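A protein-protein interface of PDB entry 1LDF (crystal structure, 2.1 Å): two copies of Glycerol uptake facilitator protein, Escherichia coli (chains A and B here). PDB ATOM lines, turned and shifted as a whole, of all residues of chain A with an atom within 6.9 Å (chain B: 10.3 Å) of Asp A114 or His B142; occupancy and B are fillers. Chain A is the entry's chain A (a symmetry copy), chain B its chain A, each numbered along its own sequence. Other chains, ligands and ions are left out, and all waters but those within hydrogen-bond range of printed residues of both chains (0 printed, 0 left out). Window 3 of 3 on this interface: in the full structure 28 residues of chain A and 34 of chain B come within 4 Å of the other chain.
No position is printed for both chains.
Of the printed residues of chain B, Ala A35 touches Pro B196. Of chain B, only His B142 (3.1 Å) comes within 4 Å of Asn A110. Printed residues of chain B within 4 Å of Leu A111: Asn B140 (3.9 Å), His B142 (3.9 Å), Ile B143 (3.8 Å) and Leu B197 (3.98 Å). Of chain B, only His B142 (2.8 Å) comes within 4 Å of Asp A114. No residue of chain B comes within 4 Å of Gln A117. His B142 touches three residues of chain A. Of the printed residues of chain A, Ile B143 touches Leu A111. Phe B145 touches none of the printed residues of chain A. The nearest residue of chain B that does not touch Asp A114 is Pro B141 (6.3 Å).
Printed residues of chain B that touch a printed residue of chain A: Asn B140, His B142, Ile B143, Pro B196 and Leu B197. Hydrophobic or aromatic side chains of chain B within 4 Å of the printed part of chain A: His B142, Ile B143, Pro B196 and Leu B197. Along chain B the printed residues that touch a printed residue of chain A span positions 140 to 197. Hydrophobic or aromatic side chains of chain A within 4 Å of the printed part of chain B: Ala A35 and Leu A111. Among the printed residues, 7 pairs touch across the chains. Among the printed residues, no Asp or Glu carboxylate lies within 4 Å of a Lys or Arg side-chain nitrogen of the other chain.
Among the printed residues, merely in contact across the chains: Ala A35 with Pro B196 (3.8 Å), Asn A110 with His B142 (3.1 Å), Leu A111 with Asn B140 (3.9 Å), Leu A111 with His B142 (3.9 Å), Leu A111 with Ile B143 (3.8 Å), Leu A111 with Leu B197 (3.98 Å) and Asp A114 with His B142 (2.8 Å).
The backbone NH (N) of His B142 sits at hydrogen-bond distance from the side-chain amide oxygen (OD1) of Asn B140. The backbone carbonyl oxygen (O) of Asp A114 sits at hydrogen-bond distance from the side-chain hydroxyl (OG1) of Thr A118, 3.1 Å away. O of Pro B196 is in hydrogen-bond range of ND2 of Asn B140, at 3.1 Å. The backbone NH (N) of Asn B140 lies within hydrogen-bond range of the backbone carbonyl oxygen (O) of Leu B197 (2.9 Å).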
ATOM      1  N   VAL A  34      33.407  -8.769  28.898  1.00  0.00           N
ATOM      2  CA  VAL A  34      33.100  -7.429  28.403  1.00  0.00           C
ATOM      3  C   VAL A  34      31.706  -6.878  28.682  1.00  0.00           C
ATOM      4  O   VAL A  34      31.424  -5.737  28.334  1.00  0.00           O
ATOM      5  CB  VAL A  34      33.360  -7.331  26.873  1.00  0.00           C
ATOM      6  CG1 VAL A  34      34.799  -7.728  26.570  1.00  0.00           C
ATOM      7  CG2 VAL A  34      32.403  -8.224  26.108  1.00  0.00           C
ATOM      8  N   ALA A  35      30.840  -7.666  29.311  1.00  0.00           N
ATOM      9  CA  ALA A  35      29.485  -7.204  29.603  1.00  0.00           C
ATOM     10  C   ALA A  35      29.219  -7.099  31.098  1.00  0.00           C
ATOM     11  O   ALA A  35      28.117  -6.766  31.510  1.00  0.00           O
ATOM     12  CB  ALA A  35      28.456  -8.136  28.951  1.00  0.00           C
ATOM     13  N   TYR A 109      30.450  -7.186  19.485  1.00  0.00           N
ATOM     14  CA  TYR A 109      31.341  -6.192  18.883  1.00  0.00           C
ATOM     15  C   TYR A 109      31.589  -4.901  19.672  1.00  0.00           C
ATOM     16  O   TYR A 109      32.722  -4.586  20.045  1.00  0.00           O
ATOM     17  CB  TYR A 109      30.795  -5.812  17.503  1.00  0.00           C
ATOM     18  CG  TYR A 109      31.731  -4.974  16.667  1.00  0.00           C
ATOM     19  CD1 TYR A 109      32.755  -5.567  15.928  1.00  0.00           C
ATOM     20  CD2 TYR A 109      31.585  -3.588  16.599  1.00  0.00           C
ATOM     21  CE1 TYR A 109      33.608  -4.803  15.132  1.00  0.00           C
ATOM     22  CE2 TYR A 109      32.433  -2.814  15.811  1.00  0.00           C
ATOM     23  CZ  TYR A 109      33.442  -3.428  15.078  1.00  0.00           C
ATOM     24  OH  TYR A 109      34.281  -2.671  14.285  1.00  0.00           O
ATOM     25  N   ASN A 110      30.523  -4.147  19.901  1.00  0.00           N
ATOM     26  CA  ASN A 110      30.607  -2.871  20.597  1.00  0.00           C
ATOM     27  C   ASN A 110      31.137  -2.953  22.014  1.00  0.00           C
ATOM     28  O   ASN A 110      31.841  -2.054  22.464  1.00  0.00           O
ATOM     29  CB  ASN A 110      29.238  -2.199  20.595  1.00  0.00           C
ATOM     30  CG  ASN A 110      28.744  -1.899  19.192  1.00  0.00           C
ATOM     31  OD1 ASN A 110      29.337  -1.098  18.472  1.00  0.00           O
ATOM     32  ND2 ASN A 110      27.655  -2.553  18.792  1.00  0.00           N
ATOM     33  N   LEU A 111      30.801  -4.024  22.722  1.00  0.00           N
ATOM     34  CA  LEU A 111      31.264  -4.176  24.093  1.00  0.00           C
ATOM     35  C   LEU A 111      32.778  -4.404  24.153  1.00  0.00           C
ATOM     36  O   LEU A 111      33.446  -3.905  25.065  1.00  0.00           O
ATOM     37  CB  LEU A 111      30.489  -5.301  24.806  1.00  0.00           C
ATOM     38  CG  LEU A 111      29.021  -4.947  25.126  1.00  0.00           C
ATOM     39  CD1 LEU A 111      28.181  -4.934  23.849  1.00  0.00           C
ATOM     40  CD2 LEU A 111      28.438  -5.961  26.097  1.00  0.00           C
ATOM     41  N   PHE A 112      33.333  -5.131  23.186  1.00  0.00           N
ATOM     42  CA  PHE A 112      34.781  -5.346  23.178  1.00  0.00           C
ATOM     43  C   PHE A 112      35.513  -4.005  23.067  1.00  0.00           C
ATOM     44  O   PHE A 112      36.368  -3.682  23.897  1.00  0.00           O
ATOM     45  CB  PHE A 112      35.216  -6.232  22.006  1.00  0.00           C
ATOM     46  CG  PHE A 112      35.100  -7.709  22.274  1.00  0.00           C
ATOM     47  CD1 PHE A 112      33.935  -8.399  21.959  1.00  0.00           C
ATOM     48  CD2 PHE A 112      36.166  -8.409  22.841  1.00  0.00           C
ATOM     49  CE1 PHE A 112      33.828  -9.768  22.203  1.00  0.00           C
ATOM     50  CE2 PHE A 112      36.070  -9.773  23.089  1.00  0.00           C
ATOM     51  CZ  PHE A 112      34.895 -10.457  22.769  1.00  0.00           C
ATOM     52  N   PHE A 113      35.171  -3.220  22.045  1.00  0.00           N
ATOM     53  CA  PHE A 113      35.823  -1.929  21.844  1.00  0.00           C
ATOM     54  C   PHE A 113      35.641  -0.952  22.997  1.00  0.00           C
ATOM     55  O   PHE A 113      36.600  -0.334  23.442  1.00  0.00           O
ATOM     56  CB  PHE A 113      35.357  -1.290  20.528  1.00  0.00           C
ATOM     57  CG  PHE A 113      35.929  -1.958  19.306  1.00  0.00           C
ATOM     58  CD1 PHE A 113      35.311  -3.077  18.749  1.00  0.00           C
ATOM     59  CD2 PHE A 113      37.126  -1.507  18.751  1.00  0.00           C
ATOM     60  CE1 PHE A 113      35.878  -3.738  17.657  1.00  0.00           C
ATOM     61  CE2 PHE A 113      37.701  -2.161  17.661  1.00  0.00           C
ATOM     62  CZ  PHE A 113      37.077  -3.278  17.113  1.00  0.00           C
ATOM     63  N   ASP A 114      34.414  -0.813  23.484  1.00  0.00           N
ATOM     64  CA  ASP A 114      34.152   0.094  24.594  1.00  0.00           C
ATOM     65  C   ASP A 114      34.919  -0.323  25.846  1.00  0.00           C
ATOM     66  O   ASP A 114      35.393   0.524  26.606  1.00  0.00           O
ATOM     67  CB  ASP A 114      32.647   0.150  24.870  1.00  0.00           C
ATOM     68  CG  ASP A 114      31.881   0.857  23.754  1.00  0.00           C
ATOM     69  OD1 ASP A 114      32.462   1.074  22.670  1.00  0.00           O
ATOM     70  OD2 ASP A 114      30.698   1.194  23.950  1.00  0.00           O
ATOM     71  N   PHE A 115      35.053  -1.629  26.054  1.00  0.00           N
ATOM     72  CA  PHE A 115      35.780  -2.143  27.210  1.00  0.00           C
ATOM     73  C   PHE A 115      37.274  -1.844  27.058  1.00  0.00           C
ATOM     74  O   PHE A 115      37.941  -1.454  28.018  1.00  0.00           O
ATOM     75  CB  PHE A 115      35.572  -3.657  27.342  1.00  0.00           C
ATOM     76  CG  PHE A 115      36.182  -4.245  28.585  1.00  0.00           C
ATOM     77  CD1 PHE A 115      35.451  -4.312  29.770  1.00  0.00           C
ATOM     78  CD2 PHE A 115      37.499  -4.706  28.581  1.00  0.00           C
ATOM     79  CE1 PHE A 115      36.022  -4.828  30.935  1.00  0.00           C
ATOM     80  CE2 PHE A 115      38.082  -5.224  29.744  1.00  0.00           C
ATOM     81  CZ  PHE A 115      37.341  -5.284  30.924  1.00  0.00           C
ATOM     82  N   GLU A 116      37.796  -2.031  25.848  1.00  0.00           N
ATOM     83  CA  GLU A 116      39.210  -1.769  25.586  1.00  0.00           C
ATOM     84  C   GLU A 116      39.508  -0.272  25.688  1.00  0.00           C
ATOM     85  O   GLU A 116      40.578   0.128  26.134  1.00  0.00           O
ATOM     86  CB  GLU A 116      39.603  -2.293  24.200  1.00  0.00           C
ATOM     87  CG  GLU A 116      39.443  -3.804  24.069  1.00  0.00           C
ATOM     88  CD  GLU A 116      39.713  -4.298  22.674  1.00  0.00           C
ATOM     89  OE1 GLU A 116      39.198  -3.679  21.716  1.00  0.00           O
ATOM     90  OE2 GLU A 116      40.433  -5.312  22.536  1.00  0.00           O
ATOM     91  N   GLN A 117      38.547   0.548  25.287  1.00  0.00           N
ATOM     92  CA  GLN A 117      38.714   1.991  25.351  1.00  0.00           C
ATOM     93  C   GLN A 117      38.722   2.424  26.817  1.00  0.00           C
ATOM     94  O   GLN A 117      39.647   3.090  27.271  1.00  0.00           O
ATOM     95  CB  GLN A 117      37.561   2.674  24.618  1.00  0.00           C
ATOM     96  CG  GLN A 117      37.776   4.145  24.324  1.00  0.00           C
ATOM     97  CD  GLN A 117      36.493   4.850  23.897  1.00  0.00           C
ATOM     98  OE1 GLN A 117      35.606   4.246  23.284  1.00  0.00           O
ATOM     99  NE2 GLN A 117      36.399   6.143  24.203  1.00  0.00           N
ATOM    100  N   THR A 118      37.687   2.021  27.552  1.00  0.00           N
ATOM    101  CA  THR A 118      37.548   2.357  28.967  1.00  0.00           C
ATOM    102  C   THR A 118      38.709   1.889  29.839  1.00  0.00           C
ATOM    103  O   THR A 118      39.144   2.615  30.723  1.00  0.00           O
ATOM    104  CB  THR A 118      36.242   1.772  29.548  1.00  0.00           C
ATOM    105  OG1 THR A 118      35.124   2.480  29.007  1.00  0.00           O
ATOM    106  CG2 THR A 118      36.220   1.897  31.063  1.00  0.00           C
ATOM    107  N   HIS A 119      39.206   0.680  29.600  1.00  0.00           N
ATOM    108  CA  HIS A 119      40.309   0.151  30.397  1.00  0.00           C
ATOM    109  C   HIS A 119      41.679   0.347  29.753  1.00  0.00           C
ATOM    110  O   HIS A 119      42.673  -0.217  30.208  1.00  0.00           O
ATOM    111  CB  HIS A 119      40.067  -1.328  30.683  1.00  0.00           C
ATOM    112  CG  HIS A 119      38.834  -1.582  31.495  1.00  0.00           C
ATOM    113  ND1 HIS A 119      38.812  -1.468  32.870  1.00  0.00           N
ATOM    114  CD2 HIS A 119      37.568  -1.888  31.123  1.00  0.00           C
ATOM    115  CE1 HIS A 119      37.585  -1.693  33.308  1.00  0.00           C
ATOM    116  NE2 HIS A 119      36.812  -1.950  32.270  1.00  0.00           N
ATOM    117  N   HIS A 120      41.728   1.150  28.696  1.00  0.00           N
ATOM    118  CA  HIS A 120      42.982   1.433  28.002  1.00  0.00           C
ATOM    119  C   HIS A 120      43.758   0.175  27.625  1.00  0.00           C
ATOM    120  O   HIS A 120      44.933   0.044  27.953  1.00  0.00           O
ATOM    121  CB  HIS A 120      43.868   2.331  28.870  1.00  0.00           C
ATOM    122  CG  HIS A 120      43.164   3.545  29.391  1.00  0.00           C
ATOM    123  ND1 HIS A 120      42.608   3.600  30.652  1.00  0.00           N
ATOM    124  CD2 HIS A 120      42.900   4.740  28.810  1.00  0.00           C
ATOM    125  CE1 HIS A 120      42.034   4.776  30.826  1.00  0.00           C
ATOM    126  NE2 HIS A 120      42.196   5.487  29.723  1.00  0.00           N
ATOM    127  N   TYR B 138      15.106  -4.982  27.276  1.00  0.00           N
ATOM    128  CA  TYR B 138      15.632  -3.735  26.748  1.00  0.00           C
ATOM    129  C   TYR B 138      17.079  -3.991  26.348  1.00  0.00           C
ATOM    130  O   TYR B 138      17.764  -4.810  26.954  1.00  0.00           O
ATOM    131  CB  TYR B 138      15.509  -2.621  27.788  1.00  0.00           C
ATOM    132  CG  TYR B 138      14.062  -2.336  28.124  1.00  0.00           C
ATOM    133  CD1 TYR B 138      13.435  -2.978  29.189  1.00  0.00           C
ATOM    134  CD2 TYR B 138      13.298  -1.472  27.332  1.00  0.00           C
ATOM    135  CE1 TYR B 138      12.078  -2.772  29.465  1.00  0.00           C
ATOM    136  CE2 TYR B 138      11.937  -1.261  27.599  1.00  0.00           C
ATOM    137  CZ  TYR B 138      11.338  -1.917  28.668  1.00  0.00           C
ATOM    138  OH  TYR B 138      10.001  -1.725  28.938  1.00  0.00           O
ATOM    139  N   PRO B 139      17.557  -3.296  25.311  1.00  0.00           N
ATOM    140  CA  PRO B 139      18.925  -3.466  24.821  1.00  0.00           C
ATOM    141  C   PRO B 139      20.033  -2.986  25.751  1.00  0.00           C
ATOM    142  O   PRO B 139      19.837  -2.086  26.564  1.00  0.00           O
ATOM    143  CB  PRO B 139      18.903  -2.697  23.504  1.00  0.00           C
ATOM    144  CG  PRO B 139      18.026  -1.529  23.851  1.00  0.00           C
ATOM    145  CD  PRO B 139      16.889  -2.172  24.624  1.00  0.00           C
ATOM    146  N   ASN B 140      21.196  -3.620  25.621  1.00  0.00           N
ATOM    147  CA  ASN B 140      22.366  -3.259  26.402  1.00  0.00           C
ATOM    148  C   ASN B 140      22.705  -1.833  25.943  1.00  0.00           C
ATOM    149  O   ASN B 140      22.506  -1.483  24.779  1.00  0.00           O
ATOM    150  CB  ASN B 140      23.515  -4.229  26.085  1.00  0.00           C
ATOM    151  CG  ASN B 140      24.815  -3.861  26.784  1.00  0.00           C
ATOM    152  OD1 ASN B 140      25.455  -2.861  26.452  1.00  0.00           O
ATOM    153  ND2 ASN B 140      25.209  -4.671  27.761  1.00  0.00           N
ATOM    154  N   PRO B 141      23.207  -0.994  26.854  1.00  0.00           N
ATOM    155  CA  PRO B 141      23.562   0.392  26.520  1.00  0.00           C
ATOM    156  C   PRO B 141      24.524   0.546  25.335  1.00  0.00           C
ATOM    157  O   PRO B 141      24.457   1.525  24.598  1.00  0.00           O
ATOM    158  CB  PRO B 141      24.177   0.911  27.820  1.00  0.00           C
ATOM    159  CG  PRO B 141      23.468   0.120  28.872  1.00  0.00           C
ATOM    160  CD  PRO B 141      23.445  -1.269  28.282  1.00  0.00           C
ATOM    161  N   HIS B 142      25.405  -0.429  25.143  1.00  0.00           N
ATOM    162  CA  HIS B 142      26.389  -0.355  24.067  1.00  0.00           C
ATOM    163  C   HIS B 142      25.972  -0.823  22.670  1.00  0.00           C
ATOM    164  O   HIS B 142      26.779  -0.764  21.747  1.00  0.00           O
ATOM    165  CB  HIS B 142      27.659  -1.112  24.471  1.00  0.00           C
ATOM    166  CG  HIS B 142      28.243  -0.673  25.779  1.00  0.00           C
ATOM    167  ND1 HIS B 142      27.836  -1.189  26.992  1.00  0.00           N
ATOM    168  CD2 HIS B 142      29.221   0.221  26.062  1.00  0.00           C
ATOM    169  CE1 HIS B 142      28.540  -0.637  27.963  1.00  0.00           C
ATOM    170  NE2 HIS B 142      29.388   0.222  27.427  1.00  0.00           N
ATOM    171  N   ILE B 143      24.742  -1.292  22.490  1.00  0.00           N
ATOM    172  CA  ILE B 143      24.339  -1.745  21.156  1.00  0.00           C
ATOM    173  C   ILE B 143      23.127  -0.993  20.632  1.00  0.00           C
ATOM    174  O   ILE B 143      22.372  -0.428  21.414  1.00  0.00           O
ATOM    175  CB  ILE B 143      24.037  -3.259  21.134  1.00  0.00           C
ATOM    176  CG1 ILE B 143      22.730  -3.556  21.866  1.00  0.00           C
ATOM    177  CG2 ILE B 143      25.179  -4.022  21.791  1.00  0.00           C
ATOM    178  CD1 ILE B 143      22.256  -4.983  21.683  1.00  0.00           C
ATOM    179  N   ASN B 144      22.943  -0.989  19.312  1.00  0.00           N
ATOM    180  CA  ASN B 144      21.811  -0.285  18.721  1.00  0.00           C
ATOM    181  C   ASN B 144      20.691  -1.210  18.262  1.00  0.00           C
ATOM    182  O   ASN B 144      20.760  -2.426  18.438  1.00  0.00           O
ATOM    183  CB  ASN B 144      22.259   0.582  17.541  1.00  0.00           C
ATOM    184  CG  ASN B 144      22.787  -0.235  16.379  1.00  0.00           C
ATOM    185  OD1 ASN B 144      22.305  -1.336  16.100  1.00  0.00           O
ATOM    186  ND2 ASN B 144      23.771   0.314  15.676  1.00  0.00           N
ATOM    187  N   PHE B 145      19.670  -0.604  17.662  1.00  0.00           N
ATOM    188  CA  PHE B 145      18.489  -1.304  17.169  1.00  0.00           C
ATOM    189  C   PHE B 145      18.801  -2.503  16.277  1.00  0.00           C
ATOM    190  O   PHE B 145      18.353  -3.611  16.550  1.00  0.00           O
ATOM    191  CB  PHE B 145      17.589  -0.329  16.398  1.00  0.00           C
ATOM    192  CG  PHE B 145      16.221  -0.873  16.096  1.00  0.00           C
ATOM    193  CD1 PHE B 145      15.185  -0.730  17.014  1.00  0.00           C
ATOM    194  CD2 PHE B 145      15.974  -1.558  14.908  1.00  0.00           C
ATOM    195  CE1 PHE B 145      13.915  -1.263  16.761  1.00  0.00           C
ATOM    196  CE2 PHE B 145      14.709  -2.098  14.640  1.00  0.00           C
ATOM    197  CZ  PHE B 145      13.675  -1.948  15.573  1.00  0.00           C
ATOM    198  N   VAL B 146      19.556  -2.272  15.206  1.00  0.00           N
ATOM    199  CA  VAL B 146      19.909  -3.332  14.263  1.00  0.00           C
ATOM    200  C   VAL B 146      20.717  -4.430  14.937  1.00  0.00           C
ATOM    201  O   VAL B 146      20.522  -5.617  14.665  1.00  0.00           O
ATOM    202  CB  VAL B 146      20.726  -2.774  13.066  1.00  0.00           C
ATOM    203  CG1 VAL B 146      21.028  -3.888  12.074  1.00  0.00           C
ATOM    204  CG2 VAL B 146      19.950  -1.666  12.383  1.00  0.00           C
ATOM    205  N   GLN B 147      21.626  -4.028  15.814  1.00  0.00           N
ATOM    206  CA  GLN B 147      22.464  -4.974  16.535  1.00  0.00           C
ATOM    207  C   GLN B 147      21.593  -5.882  17.406  1.00  0.00           C
ATOM    208  O   GLN B 147      21.799  -7.094  17.461  1.00  0.00           O
ATOM    209  CB  GLN B 147      23.453  -4.221  17.422  1.00  0.00           C
ATOM    210  CG  GLN B 147      24.471  -5.120  18.097  1.00  0.00           C
ATOM    211  CD  GLN B 147      25.493  -5.656  17.119  1.00  0.00           C
ATOM    212  OE1 GLN B 147      26.267  -6.563  17.435  1.00  0.00           O
ATOM    213  NE2 GLN B 147      25.510  -5.084  15.919  1.00  0.00           N
ATOM    214  N   ALA B 148      20.622  -5.278  18.090  1.00  0.00           N
ATOM    215  CA  ALA B 148      19.712  -6.013  18.963  1.00  0.00           C
ATOM    216  C   ALA B 148      18.812  -6.923  18.137  1.00  0.00           C
ATOM    217  O   ALA B 148      18.471  -8.028  18.566  1.00  0.00           O
ATOM    218  CB  ALA B 148      18.865  -5.039  19.778  1.00  0.00           C
ATOM    219  N   VAL B 151      20.669 -10.137  17.278  1.00  0.00           N
ATOM    220  CA  VAL B 151      20.741 -11.047  18.425  1.00  0.00           C
ATOM    221  C   VAL B 151      19.464 -11.881  18.577  1.00  0.00           C
ATOM    222  O   VAL B 151      19.519 -13.113  18.644  1.00  0.00           O
ATOM    223  CB  VAL B 151      20.982 -10.263  19.746  1.00  0.00           C
ATOM    224  CG1 VAL B 151      20.987 -11.219  20.931  1.00  0.00           C
ATOM    225  CG2 VAL B 151      22.295  -9.509  19.670  1.00  0.00           C
ATOM    226  N   PRO B 196      23.002 -10.687  28.399  1.00  0.00           N
ATOM    227  CA  PRO B 196      23.491  -9.318  28.629  1.00  0.00           C
ATOM    228  C   PRO B 196      23.268  -8.367  27.461  1.00  0.00           C
ATOM    229  O   PRO B 196      23.317  -7.146  27.631  1.00  0.00           O
ATOM    230  CB  PRO B 196      24.974  -9.532  28.932  1.00  0.00           C
ATOM    231  CG  PRO B 196      24.964 -10.859  29.651  1.00  0.00           C
ATOM    232  CD  PRO B 196      24.018 -11.682  28.788  1.00  0.00           C
ATOM    233  N   LEU B 197      23.008  -8.918  26.277  1.00  0.00           N
ATOM    234  CA  LEU B 197      22.795  -8.088  25.095  1.00  0.00           C
ATOM    235  C   LEU B 197      21.365  -7.563  24.915  1.00  0.00           C
ATOM    236  O   LEU B 197      21.154  -6.351  24.775  1.00  0.00           O
ATOM    237  CB  LEU B 197      23.218  -8.850  23.835  1.00  0.00           C
ATOM    238  CG  LEU B 197      24.712  -9.181  23.693  1.00  0.00           C
ATOM    239  CD1 LEU B 197      24.956  -9.897  22.368  1.00  0.00           C
ATOM    240  CD2 LEU B 197      25.538  -7.905  23.753  1.00  0.00           C
ATOM    241  N   THR B 198      20.385  -8.464  24.912  1.00  0.00           N
ATOM    242  CA  THR B 198      19.000  -8.047  24.719  1.00  0.00           C
ATOM    243  C   THR B 198      18.003  -8.655  25.701  1.00  0.00           C
ATOM    244  O   THR B 198      16.799  -8.457  25.549  1.00  0.00           O
ATOM    245  CB  THR B 198      18.503  -8.413  23.313  1.00  0.00           C
ATOM    246  OG1 THR B 198      18.432  -9.840  23.198  1.00  0.00           O
ATOM    247  CG2 THR B 198      19.437  -7.861  22.250  1.00  0.00           C
ATOM    248  N   ARG B 228      14.825   4.897  23.540  1.00  0.00           N
ATOM    249  CA  ARG B 228      15.646   4.942  22.332  1.00  0.00           C
ATOM    250  C   ARG B 228      14.934   5.651  21.176  1.00  0.00           C
ATOM    251  O   ARG B 228      13.705   5.737  21.153  1.00  0.00           O
ATOM    252  CB  ARG B 228      16.003   3.516  21.912  1.00  0.00           C
ATOM    253  CG  ARG B 228      16.396   2.620  23.077  1.00  0.00           C
ATOM    254  CD  ARG B 228      17.840   2.810  23.506  1.00  0.00           C
ATOM    255  NE  ARG B 228      18.739   2.246  22.509  1.00  0.00           N
ATOM    256  CZ  ARG B 228      19.882   1.628  22.783  1.00  0.00           C
ATOM    257  NH1 ARG B 228      20.295   1.483  24.034  1.00  0.00           N
ATOM    258  NH2 ARG B 228      20.604   1.136  21.793  1.00  0.00           N
